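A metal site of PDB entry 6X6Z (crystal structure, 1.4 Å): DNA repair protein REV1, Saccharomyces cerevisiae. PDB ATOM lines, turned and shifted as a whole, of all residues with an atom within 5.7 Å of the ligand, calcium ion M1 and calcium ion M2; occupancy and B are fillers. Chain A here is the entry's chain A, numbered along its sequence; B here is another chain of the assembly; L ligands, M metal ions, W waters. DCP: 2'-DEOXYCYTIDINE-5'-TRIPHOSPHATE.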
ATOM      1  N   ARG A  20      25.415  -1.890 -25.090  1.00  0.00           N
ATOM      2  CA  ARG A  20      25.257  -3.228 -24.540  1.00  0.00           C
ATOM      3  C   ARG A  20      24.064  -3.323 -23.595  1.00  0.00           C
ATOM      4  O   ARG A  20      23.463  -4.396 -23.474  1.00  0.00           O
ATOM      5  CB  ARG A  20      26.553  -3.736 -23.892  1.00  0.00           C
ATOM      6  CG  ARG A  20      26.621  -3.635 -22.370  1.00  0.00           C
ATOM      7  CD  ARG A  20      27.123  -2.274 -21.894  1.00  0.00           C
ATOM      8  NE  ARG A  20      27.322  -2.312 -20.451  1.00  0.00           N
ATOM      9  CZ  ARG A  20      27.591  -1.259 -19.690  1.00  0.00           C
ATOM     10  NH1 ARG A  20      27.665  -0.033 -20.221  1.00  0.00           N
ATOM     11  NH2 ARG A  20      27.776  -1.413 -18.384  1.00  0.00           N
ATOM     12  N   LEU A  21      23.726  -2.235 -22.913  1.00  0.00           N
ATOM     13  CA  LEU A  21      22.561  -2.249 -22.021  1.00  0.00           C
ATOM     14  C   LEU A  21      21.264  -2.360 -22.812  1.00  0.00           C
ATOM     15  O   LEU A  21      20.343  -3.074 -22.399  1.00  0.00           O
ATOM     16  CB  LEU A  21      22.583  -1.029 -21.097  1.00  0.00           C
ATOM     17  CG  LEU A  21      23.786  -0.985 -20.169  1.00  0.00           C
ATOM     18  CD1 LEU A  21      23.791   0.349 -19.408  1.00  0.00           C
ATOM     19  CD2 LEU A  21      23.795  -2.174 -19.200  1.00  0.00           C
ATOM     20  N   LEU A  24      21.167  -6.096 -23.694  1.00  0.00           N
ATOM     21  CA  LEU A  24      20.723  -6.913 -22.563  1.00  0.00           C
ATOM     22  C   LEU A  24      19.205  -6.900 -22.443  1.00  0.00           C
ATOM     23  O   LEU A  24      18.562  -7.943 -22.297  1.00  0.00           O
ATOM     24  CB  LEU A  24      21.349  -6.444 -21.257  1.00  0.00           C
ATOM     25  CG  LEU A  24      22.828  -6.653 -20.992  1.00  0.00           C
ATOM     26  CD1 LEU A  24      23.158  -6.153 -19.585  1.00  0.00           C
ATOM     27  CD2 LEU A  24      23.199  -8.130 -21.138  1.00  0.00           C
ATOM     28  N   ASP A  58      24.580 -19.815 -14.622  1.00  0.00           N
ATOM     29  CA  ASP A  58      24.973 -18.502 -15.120  1.00  0.00           C
ATOM     30  C   ASP A  58      26.395 -18.556 -15.682  1.00  0.00           C
ATOM     31  O   ASP A  58      27.279 -19.161 -15.067  1.00  0.00           O
ATOM     32  CB  ASP A  58      24.854 -17.488 -13.965  1.00  0.00           C
ATOM     33  CG  ASP A  58      25.506 -16.153 -14.298  1.00  0.00           C
ATOM     34  OD1 ASP A  58      24.808 -15.228 -14.797  1.00  0.00           O
ATOM     35  OD2 ASP A  58      26.728 -16.060 -14.052  1.00  0.00           O
ATOM     36  N   PHE A  59      26.600 -17.926 -16.841  1.00  0.00           N
ATOM     37  CA  PHE A  59      27.942 -17.914 -17.447  1.00  0.00           C
ATOM     38  C   PHE A  59      28.886 -17.084 -16.589  1.00  0.00           C
ATOM     39  O   PHE A  59      28.567 -15.949 -16.196  1.00  0.00           O
ATOM     40  CB  PHE A  59      27.929 -17.218 -18.820  1.00  0.00           C
ATOM     41  CG  PHE A  59      27.427 -18.041 -19.990  1.00  0.00           C
ATOM     42  CD1 PHE A  59      26.073 -18.230 -20.187  1.00  0.00           C
ATOM     43  CD2 PHE A  59      28.322 -18.491 -20.975  1.00  0.00           C
ATOM     44  CE1 PHE A  59      25.606 -18.901 -21.314  1.00  0.00           C
ATOM     45  CE2 PHE A  59      27.851 -19.153 -22.103  1.00  0.00           C
ATOM     46  CZ  PHE A  59      26.495 -19.363 -22.272  1.00  0.00           C
ATOM     47  N   ASP A  60      30.085 -17.610 -16.352  1.00  0.00           N
ATOM     48  CA  ASP A  60      31.137 -16.817 -15.730  1.00  0.00           C
ATOM     49  C   ASP A  60      31.600 -15.712 -16.681  1.00  0.00           C
ATOM     50  O   ASP A  60      31.823 -15.954 -17.874  1.00  0.00           O
ATOM     51  CB  ASP A  60      32.336 -17.709 -15.397  1.00  0.00           C
ATOM     52  CG  ASP A  60      31.970 -18.837 -14.476  1.00  0.00           C
ATOM     53  OD1 ASP A  60      31.221 -18.582 -13.532  1.00  0.00           O
ATOM     54  OD2 ASP A  60      32.431 -19.981 -14.721  1.00  0.00           O
ATOM     55  N   CYS A  61      31.758 -14.504 -16.124  1.00  0.00           N
ATOM     56  CA  CYS A  61      32.184 -13.295 -16.842  1.00  0.00           C
ATOM     57  C   CYS A  61      31.804 -13.340 -18.318  1.00  0.00           C
ATOM     58  O   CYS A  61      32.670 -13.362 -19.196  1.00  0.00           O
ATOM     59  CB  CYS A  61      33.679 -13.006 -16.653  1.00  0.00           C
ATOM     60  SG  CYS A  61      34.832 -14.376 -16.989  1.00  0.00           S
ATOM     61  N   PHE A  62      30.495 -13.326 -18.578  1.00  0.00           N
ATOM     62  CA  PHE A  62      29.955 -13.744 -19.868  1.00  0.00           C
ATOM     63  C   PHE A  62      30.599 -13.032 -21.061  1.00  0.00           C
ATOM     64  O   PHE A  62      31.158 -13.675 -21.949  1.00  0.00           O
ATOM     65  CB  PHE A  62      28.437 -13.578 -19.857  1.00  0.00           C
ATOM     66  CG  PHE A  62      27.769 -13.923 -21.147  1.00  0.00           C
ATOM     67  CD1 PHE A  62      27.948 -15.166 -21.733  1.00  0.00           C
ATOM     68  CD2 PHE A  62      26.927 -13.008 -21.767  1.00  0.00           C
ATOM     69  CE1 PHE A  62      27.306 -15.487 -22.916  1.00  0.00           C
ATOM     70  CE2 PHE A  62      26.285 -13.329 -22.950  1.00  0.00           C
ATOM     71  CZ  PHE A  62      26.468 -14.570 -23.527  1.00  0.00           C
ATOM     72  N   PHE A  63      30.486 -11.700 -21.132  1.00  0.00           N
ATOM     73  CA  PHE A  63      31.033 -11.008 -22.298  1.00  0.00           C
ATOM     74  C   PHE A  63      32.548 -11.212 -22.401  1.00  0.00           C
ATOM     75  O   PHE A  63      33.085 -11.344 -23.495  1.00  0.00           O
ATOM     76  CB  PHE A  63      30.769  -9.502 -22.265  1.00  0.00           C
ATOM     77  CG  PHE A  63      29.357  -9.072 -22.605  1.00  0.00           C
ATOM     78  CD1 PHE A  63      28.299  -9.972 -22.731  1.00  0.00           C
ATOM     79  CD2 PHE A  63      29.092  -7.711 -22.768  1.00  0.00           C
ATOM     80  CE1 PHE A  63      27.008  -9.509 -23.001  1.00  0.00           C
ATOM     81  CE2 PHE A  63      27.825  -7.262 -23.046  1.00  0.00           C
ATOM     82  CZ  PHE A  63      26.776  -8.148 -23.168  1.00  0.00           C
ATOM     83  N   ALA A  64      33.254 -11.209 -21.262  1.00  0.00           N
ATOM     84  CA  ALA A  64      34.715 -11.376 -21.313  1.00  0.00           C
ATOM     85  C   ALA A  64      35.070 -12.748 -21.866  1.00  0.00           C
ATOM     86  O   ALA A  64      35.976 -12.861 -22.700  1.00  0.00           O
ATOM     87  CB  ALA A  64      35.339 -11.147 -19.933  1.00  0.00           C
ATOM     88  N   ILE A  96      33.367  -0.850 -18.258  1.00  0.00           N
ATOM     89  CA  ILE A  96      33.754  -2.245 -18.349  1.00  0.00           C
ATOM     90  C   ILE A  96      32.472  -3.061 -18.250  1.00  0.00           C
ATOM     91  O   ILE A  96      31.890  -3.188 -17.172  1.00  0.00           O
ATOM     92  CB  ILE A  96      34.759  -2.629 -17.250  1.00  0.00           C
ATOM     93  CG1 ILE A  96      36.095  -1.940 -17.540  1.00  0.00           C
ATOM     94  CG2 ILE A  96      34.926  -4.152 -17.144  1.00  0.00           C
ATOM     95  CD1 ILE A  96      36.993  -1.807 -16.339  1.00  0.00           C
ATOM     96  N   ALA A  97      32.003  -3.586 -19.384  1.00  0.00           N
ATOM     97  CA  ALA A  97      30.773  -4.377 -19.349  1.00  0.00           C
ATOM     98  C   ALA A  97      31.006  -5.692 -18.606  1.00  0.00           C
ATOM     99  O   ALA A  97      30.152  -6.144 -17.828  1.00  0.00           O
ATOM    100  CB  ALA A  97      30.271  -4.629 -20.758  1.00  0.00           C
ATOM    101  N   SER A  98      32.149  -6.311 -18.854  1.00  0.00           N
ATOM    102  CA  SER A  98      32.527  -7.570 -18.203  1.00  0.00           C
ATOM    103  C   SER A  98      34.044  -7.603 -18.049  1.00  0.00           C
ATOM    104  O   SER A  98      34.719  -7.097 -18.888  1.00  0.00           O
ATOM    105  CB  SER A  98      32.002  -8.773 -18.980  1.00  0.00           C
ATOM    106  OG  SER A  98      32.282  -9.981 -18.327  1.00  0.00           O
ATOM    107  N   CYS A  99      34.485  -8.177 -16.949  1.00  0.00           N
ATOM    108  CA  CYS A  99      35.925  -8.369 -16.703  1.00  0.00           C
ATOM    109  C   CYS A  99      36.133  -9.833 -16.290  1.00  0.00           C
ATOM    110  O   CYS A  99      35.292 -10.383 -15.656  1.00  0.00           O
ATOM    111  CB  CYS A  99      36.506  -7.380 -15.706  1.00  0.00           C
ATOM    112  SG  CYS A  99      35.703  -7.377 -14.088  1.00  0.00           S
ATOM    113  N   TYR A 101      38.240 -13.050 -14.305  1.00  0.00           N
ATOM    114  CA  TYR A 101      38.558 -13.218 -12.892  1.00  0.00           C
ATOM    115  C   TYR A 101      39.989 -12.818 -12.560  1.00  0.00           C
ATOM    116  O   TYR A 101      40.264 -12.474 -11.410  1.00  0.00           O
ATOM    117  CB  TYR A 101      38.148 -14.611 -12.403  1.00  0.00           C
ATOM    118  CG  TYR A 101      36.648 -14.672 -12.163  1.00  0.00           C
ATOM    119  CD1 TYR A 101      35.755 -14.776 -13.226  1.00  0.00           C
ATOM    120  CD2 TYR A 101      36.128 -14.610 -10.882  1.00  0.00           C
ATOM    121  CE1 TYR A 101      34.373 -14.797 -13.006  1.00  0.00           C
ATOM    122  CE2 TYR A 101      34.749 -14.641 -10.661  1.00  0.00           C
ATOM    123  CZ  TYR A 101      33.882 -14.736 -11.716  1.00  0.00           C
ATOM    124  OH  TYR A 101      32.523 -14.769 -11.459  1.00  0.00           O
ATOM    125  N   ARG A 104      39.449  -9.269 -11.766  1.00  0.00           N
ATOM    126  CA  ARG A 104      38.795  -9.115 -10.485  1.00  0.00           C
ATOM    127  C   ARG A 104      39.738  -9.370  -9.317  1.00  0.00           C
ATOM    128  O   ARG A 104      39.479  -8.869  -8.215  1.00  0.00           O
ATOM    129  CB  ARG A 104      37.569 -10.030 -10.405  1.00  0.00           C
ATOM    130  CG  ARG A 104      36.543  -9.694 -11.483  1.00  0.00           C
ATOM    131  CD  ARG A 104      35.349 -10.632 -11.446  1.00  0.00           C
ATOM    132  NE  ARG A 104      34.546 -10.490 -12.659  1.00  0.00           N
ATOM    133  CZ  ARG A 104      33.294 -10.894 -12.770  1.00  0.00           C
ATOM    134  NH1 ARG A 104      32.677 -11.467 -11.731  1.00  0.00           N
ATOM    135  NH2 ARG A 104      32.645 -10.730 -13.925  1.00  0.00           N
ATOM    136  N   ASN A 110      32.672  -5.300 -12.848  1.00  0.00           N
ATOM    137  CA  ASN A 110      31.790  -4.873 -13.935  1.00  0.00           C
ATOM    138  C   ASN A 110      31.162  -3.538 -13.582  1.00  0.00           C
ATOM    139  O   ASN A 110      30.753  -3.319 -12.443  1.00  0.00           O
ATOM    140  CB  ASN A 110      30.660  -5.884 -14.127  1.00  0.00           C
ATOM    141  CG  ASN A 110      31.118  -7.203 -14.718  1.00  0.00           C
ATOM    142  OD1 ASN A 110      32.295  -7.402 -15.032  1.00  0.00           O
ATOM    143  ND2 ASN A 110      30.162  -8.112 -14.878  1.00  0.00           N
ATOM    144  N   GLY A 111      31.075  -2.650 -14.565  1.00  0.00           N
ATOM    145  CA  GLY A 111      30.495  -1.337 -14.378  1.00  0.00           C
ATOM    146  C   GLY A 111      31.498  -0.238 -14.087  1.00  0.00           C
ATOM    147  O   GLY A 111      31.149   0.940 -14.183  1.00  0.00           O
ATOM    148  N   TYR A 132      33.336  -5.580 -28.049  1.00  0.00           N
ATOM    149  CA  TYR A 132      32.122  -6.374 -27.942  1.00  0.00           C
ATOM    150  C   TYR A 132      31.952  -7.246 -29.181  1.00  0.00           C
ATOM    151  O   TYR A 132      32.294  -6.842 -30.303  1.00  0.00           O
ATOM    152  CB  TYR A 132      30.927  -5.451 -27.856  1.00  0.00           C
ATOM    153  CG  TYR A 132      30.833  -4.594 -26.613  1.00  0.00           C
ATOM    154  CD1 TYR A 132      31.398  -3.325 -26.577  1.00  0.00           C
ATOM    155  CD2 TYR A 132      30.127  -5.025 -25.504  1.00  0.00           C
ATOM    156  CE1 TYR A 132      31.276  -2.515 -25.457  1.00  0.00           C
ATOM    157  CE2 TYR A 132      30.003  -4.224 -24.371  1.00  0.00           C
ATOM    158  CZ  TYR A 132      30.572  -2.966 -24.356  1.00  0.00           C
ATOM    159  OH  TYR A 132      30.441  -2.169 -23.241  1.00  0.00           O
ATOM    160  N   SER A 161      18.371 -13.905 -17.899  1.00  0.00           N
ATOM    161  CA  SER A 161      19.187 -12.989 -18.675  1.00  0.00           C
ATOM    162  C   SER A 161      19.725 -13.748 -19.867  1.00  0.00           C
ATOM    163  O   SER A 161      19.587 -14.971 -19.958  1.00  0.00           O
ATOM    164  CB  SER A 161      20.378 -12.531 -17.836  1.00  0.00           C
ATOM    165  OG  SER A 161      20.880 -11.285 -18.282  1.00  0.00           O
ATOM    166  N   ILE A 162      20.378 -12.998 -20.757  1.00  0.00           N
ATOM    167  CA  ILE A 162      21.111 -13.604 -21.870  1.00  0.00           C
ATOM    168  C   ILE A 162      21.970 -14.784 -21.418  1.00  0.00           C
ATOM    169  O   ILE A 162      22.109 -15.773 -22.149  1.00  0.00           O
ATOM    170  CB  ILE A 162      21.944 -12.511 -22.577  1.00  0.00           C
ATOM    171  CG1 ILE A 162      22.615 -13.049 -23.855  1.00  0.00           C
ATOM    172  CG2 ILE A 162      22.998 -11.894 -21.638  1.00  0.00           C
ATOM    173  CD1 ILE A 162      21.625 -13.274 -24.994  1.00  0.00           C
ATOM    174  N   ASP A 163      22.529 -14.722 -20.210  1.00  0.00           N
ATOM    175  CA  ASP A 163      23.515 -15.692 -19.772  1.00  0.00           C
ATOM    176  C   ASP A 163      23.099 -16.462 -18.518  1.00  0.00           C
ATOM    177  O   ASP A 163      23.958 -17.074 -17.866  1.00  0.00           O
ATOM    178  CB  ASP A 163      24.867 -15.005 -19.529  1.00  0.00           C
ATOM    179  CG  ASP A 163      24.922 -14.305 -18.189  1.00  0.00           C
ATOM    180  OD1 ASP A 163      23.890 -13.746 -17.769  1.00  0.00           O
ATOM    181  OD2 ASP A 163      26.004 -14.304 -17.555  1.00  0.00           O
ATOM    182  N   GLU A 164      21.815 -16.436 -18.196  1.00  0.00           N
ATOM    183  CA  GLU A 164      21.413 -16.934 -16.868  1.00  0.00           C
ATOM    184  C   GLU A 164      19.993 -17.496 -16.879  1.00  0.00           C
ATOM    185  O   GLU A 164      19.126 -16.871 -17.406  1.00  0.00           O
ATOM    186  CB  GLU A 164      21.575 -15.740 -15.917  1.00  0.00           C
ATOM    187  CG  GLU A 164      21.325 -15.969 -14.435  1.00  0.00           C
ATOM    188  CD  GLU A 164      21.592 -14.685 -13.675  1.00  0.00           C
ATOM    189  OE1 GLU A 164      21.358 -14.719 -12.443  1.00  0.00           O
ATOM    190  OE2 GLU A 164      22.072 -13.663 -14.268  1.00  0.00           O
ATOM    191  N   LYS A 221      31.362 -19.467  -7.871  1.00  0.00           N
ATOM    192  CA  LYS A 221      32.126 -18.857  -8.942  1.00  0.00           C
ATOM    193  C   LYS A 221      33.588 -18.675  -8.548  1.00  0.00           C
ATOM    194  O   LYS A 221      33.909 -18.494  -7.364  1.00  0.00           O
ATOM    195  CB  LYS A 221      31.529 -17.511  -9.316  1.00  0.00           C
ATOM    196  CG  LYS A 221      30.289 -17.670 -10.181  1.00  0.00           C
ATOM    197  CD  LYS A 221      29.619 -16.355 -10.446  1.00  0.00           C
ATOM    198  CE  LYS A 221      28.532 -16.513 -11.507  1.00  0.00           C
ATOM    199  NZ  LYS A 221      29.131 -16.616 -12.884  1.00  0.00           N
ATOM    200  P    DG B  12      18.672 -10.218 -12.243  1.00  0.00           P
ATOM    201  OP1  DG B  12      17.279 -10.475 -12.486  1.00  0.00           O
ATOM    202  OP2  DG B  12      19.377 -10.777 -11.147  1.00  0.00           O
ATOM    203  O5'  DG B  12      19.446 -10.618 -13.575  1.00  0.00           O
ATOM    204  C5'  DG B  12      20.850 -10.571 -13.609  1.00  0.00           C
ATOM    205  C4'  DG B  12      21.251  -9.870 -14.887  1.00  0.00           C
ATOM    206  O4'  DG B  12      20.992  -8.472 -14.733  1.00  0.00           O
ATOM    207  C3'  DG B  12      22.736  -9.934 -15.206  1.00  0.00           C
ATOM    208  O3'  DG B  12      22.936 -10.944 -16.165  1.00  0.00           O
ATOM    209  C2'  DG B  12      22.971  -8.665 -16.003  1.00  0.00           C
ATOM    210  C1'  DG B  12      21.735  -7.811 -15.704  1.00  0.00           C
ATOM    211  N9   DG B  12      22.005  -6.475 -15.237  1.00  0.00           N
ATOM    212  C8   DG B  12      22.930  -6.050 -14.322  1.00  0.00           C
ATOM    213  N7   DG B  12      22.943  -4.761 -14.162  1.00  0.00           N
ATOM    214  C5   DG B  12      21.935  -4.303 -15.004  1.00  0.00           C
ATOM    215  C6   DG B  12      21.482  -2.989 -15.282  1.00  0.00           C
ATOM    216  O6   DG B  12      21.881  -1.927 -14.821  1.00  0.00           O
ATOM    217  N1   DG B  12      20.455  -2.984 -16.203  1.00  0.00           N
ATOM    218  C2   DG B  12      19.932  -4.104 -16.796  1.00  0.00           C
ATOM    219  N2   DG B  12      18.966  -3.898 -17.685  1.00  0.00           N
ATOM    220  N3   DG B  12      20.354  -5.325 -16.567  1.00  0.00           N
ATOM    221  C4   DG B  12      21.350  -5.352 -15.672  1.00  0.00           C
HETATM  222  N1  DCP L   1      26.781  -6.492 -17.993  1.00  0.00           N
HETATM  223  C2  DCP L   1      27.082  -5.110 -18.383  1.00  0.00           C
HETATM  224  N3  DCP L   1      27.226  -4.096 -17.330  1.00  0.00           N
HETATM  225  C4  DCP L   1      27.081  -4.475 -15.958  1.00  0.00           C
HETATM  226  C5  DCP L   1      26.771  -5.860 -15.563  1.00  0.00           C
HETATM  227  C6  DCP L   1      26.610  -6.879 -16.607  1.00  0.00           C
HETATM  228  O2  DCP L   1      27.195  -4.868 -19.521  1.00  0.00           O
HETATM  229  N4  DCP L   1      27.237  -3.470 -14.953  1.00  0.00           N
HETATM  230  C1' DCP L   1      26.700  -7.402 -19.087  1.00  0.00           C
HETATM  231  C2' DCP L   1      27.903  -7.959 -19.341  1.00  0.00           C
HETATM  232  C3' DCP L   1      27.921  -9.319 -18.476  1.00  0.00           C
HETATM  233  C4' DCP L   1      26.640  -9.810 -18.669  1.00  0.00           C
HETATM  234  O4' DCP L   1      25.769  -8.560 -18.623  1.00  0.00           O
HETATM  235  O3' DCP L   1      28.948 -10.229 -18.913  1.00  0.00           O
HETATM  236  C5' DCP L   1      26.106 -10.711 -17.558  1.00  0.00           C
HETATM  237  O5' DCP L   1      26.070 -10.025 -16.329  1.00  0.00           O
HETATM  238  PA  DCP L   1      26.480 -10.809 -14.969  1.00  0.00           P
HETATM  239  O1A DCP L   1      26.010  -9.987 -13.811  1.00  0.00           O
HETATM  240  O2A DCP L   1      26.038 -12.248 -15.007  1.00  0.00           O
HETATM  241  O3A DCP L   1      28.105 -10.715 -14.915  1.00  0.00           O
HETATM  242  PB  DCP L   1      29.248 -11.589 -15.662  1.00  0.00           P
HETATM  243  O1B DCP L   1      30.119 -10.656 -16.456  1.00  0.00           O
HETATM  244  O2B DCP L   1      28.677 -12.753 -16.392  1.00  0.00           O
HETATM  245  O3B DCP L   1      30.189 -12.116 -14.436  1.00  0.00           O
HETATM  246  PG  DCP L   1      29.764 -13.157 -13.247  1.00  0.00           P
HETATM  247  O1G DCP L   1      30.766 -14.293 -13.356  1.00  0.00           O
HETATM  248  O2G DCP L   1      29.920 -12.382 -11.959  1.00  0.00           O
HETATM  249  O3G DCP L   1      28.363 -13.618 -13.513  1.00  0.00           O
HETATM  250 CA    CA M   1      27.131 -14.247 -15.513  1.00  0.00          CA
HETATM  251 CA    CA M   2      23.904 -13.173 -15.439  1.00  0.00          CA
HETATM  252  O   HOH W   1      26.808  -3.966 -12.162  1.00  0.00           O
HETATM  253  O   HOH W   2      26.313 -13.557 -11.619  1.00  0.00           O
HETATM  254  O   HOH W   3      26.507 -10.882 -11.085  1.00  0.00           O
HETATM  255  O   HOH W   4      27.801  -8.043 -13.053  1.00  0.00           O
HETATM  256  O   HOH W   5      29.588  -9.649 -11.604  1.00  0.00           O
HETATM  257  O   HOH W   6      23.999 -12.413 -12.566  1.00  0.00           O
HETATM  258  O   HOH W   7      29.166 -12.903  -9.414  1.00  0.00           O
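O2B of the ligand binds calcium ion M1 (2.3 Å).
The backbone carbonyl oxygen (O) of Phe 59 binds calcium ion M1 (2.3 Å).
Calcium ion M1 is bound by OD2 of Asp 163 (2.3 Å).
An oxygen (O2A) of the ligand binds calcium ion M1.
The side-chain carboxylate (OD2) of Asp 58 binds calcium ion M1 (2.4 Å).
Calcium ion M1 is bound by an oxygen (O3G) of the ligand (2.4 Å).
OD1 of Asp 58 binds calcium ion M1, 2.6 Å away.
Calcium ion M1 has seven donor atoms within binding distance.
Water W4 lies within hydrogen-bond range of an oxygen (O1A) of the ligand (2.7 Å) and the side-chain amide nitrogen of Asn 110 (3.0 Å).
Calcium ion M2 is bound by OE2 of Glu 164, OD1 of Asp 58, O2A of the ligand, OD1 of Asp 163 and O3' of DG 12 of chain B.
Slightly farther from calcium ion M2 lies water W6 (3.0 Å).
The side-chain amino group (NZ) of Lys 221 sits close to the backbone carbonyl oxygen (O) of Phe 59, at 3.4 Å.
OD2 of Asp 58 lies close to NZ of Lys 221.
O3' of DG 12 of chain B sits close to OG of Ser 161.
O of Cys 99 sits at hydrogen-bond distance from NE of Arg 104, 3.1 Å away.
NZ of Lys 221 lies within salt-bridge range of OD1 of Asp 60 (2.9 Å).
The backbone NH (N) of Ala 64 sits at hydrogen-bond distance from the side-chain hydroxyl (OG) of Ser 98, 3.3 Å away.
The backbone NH (N) of Cys 99 lies within hydrogen-bond range of the side-chain amide oxygen (OD1) of Asn 110 (3.0 Å).
O of Ile 96 sits at hydrogen-bond distance from N of Gly 111, 2.8 Å away.
O1G of the ligand sits at hydrogen-bond distance from OH of Tyr 101, at 2.6 Å.
NE of Arg 20 lies within hydrogen-bond range of O2 of the ligand (2.7 Å).
The guanidinium group (NH1) of Arg 104 lies within salt-bridge range of an oxygen (O2G) of the ligand, 2.9 Å away.
NZ of Lys 221 lies within salt-bridge range of O1G of the ligand, 2.9 Å away.
An oxygen (O1B) of the ligand sits at hydrogen-bond distance from the backbone NH (N) of Phe 62 (3.4 Å).
The side-chain hydroxyl of Ser 98 sits at hydrogen-bond distance from an oxygen (O1B) of the ligand, at 2.9 Å.
N of Cys 61 lies within hydrogen-bond range of O1G of the ligand.
The side-chain amide nitrogen (ND2) of Asn 110 lies within hydrogen-bond range of an oxygen (O1B) of the ligand.
An oxygen (O3') of the ligand is in hydrogen-bond range of the backbone NH (N) of Phe 63, at 3.1 Å.
Within 4 Å of calcium ion M2: Asp 58, Asp 163, Glu 164 and DG 12 of chain B.
O of Ala 97 sits close to N1 of the ligand, at 3.4 Å.
Merely in contact with the ligand: Asp 60 (3.5 Å), Leu 24 (3.6 Å) and Gly 111 (3.9 Å).
Hydrophobic or aromatic side chains that line the ligand: Leu 24, Phe 62, Phe 63, Ala 97 and Tyr 101.
Within 4 Å of calcium ion M1: Asp 58, Phe 59 and Asp 163.
The nearest printed residue that does not touch calcium ion M1 is Lys 221 (4.1 Å).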
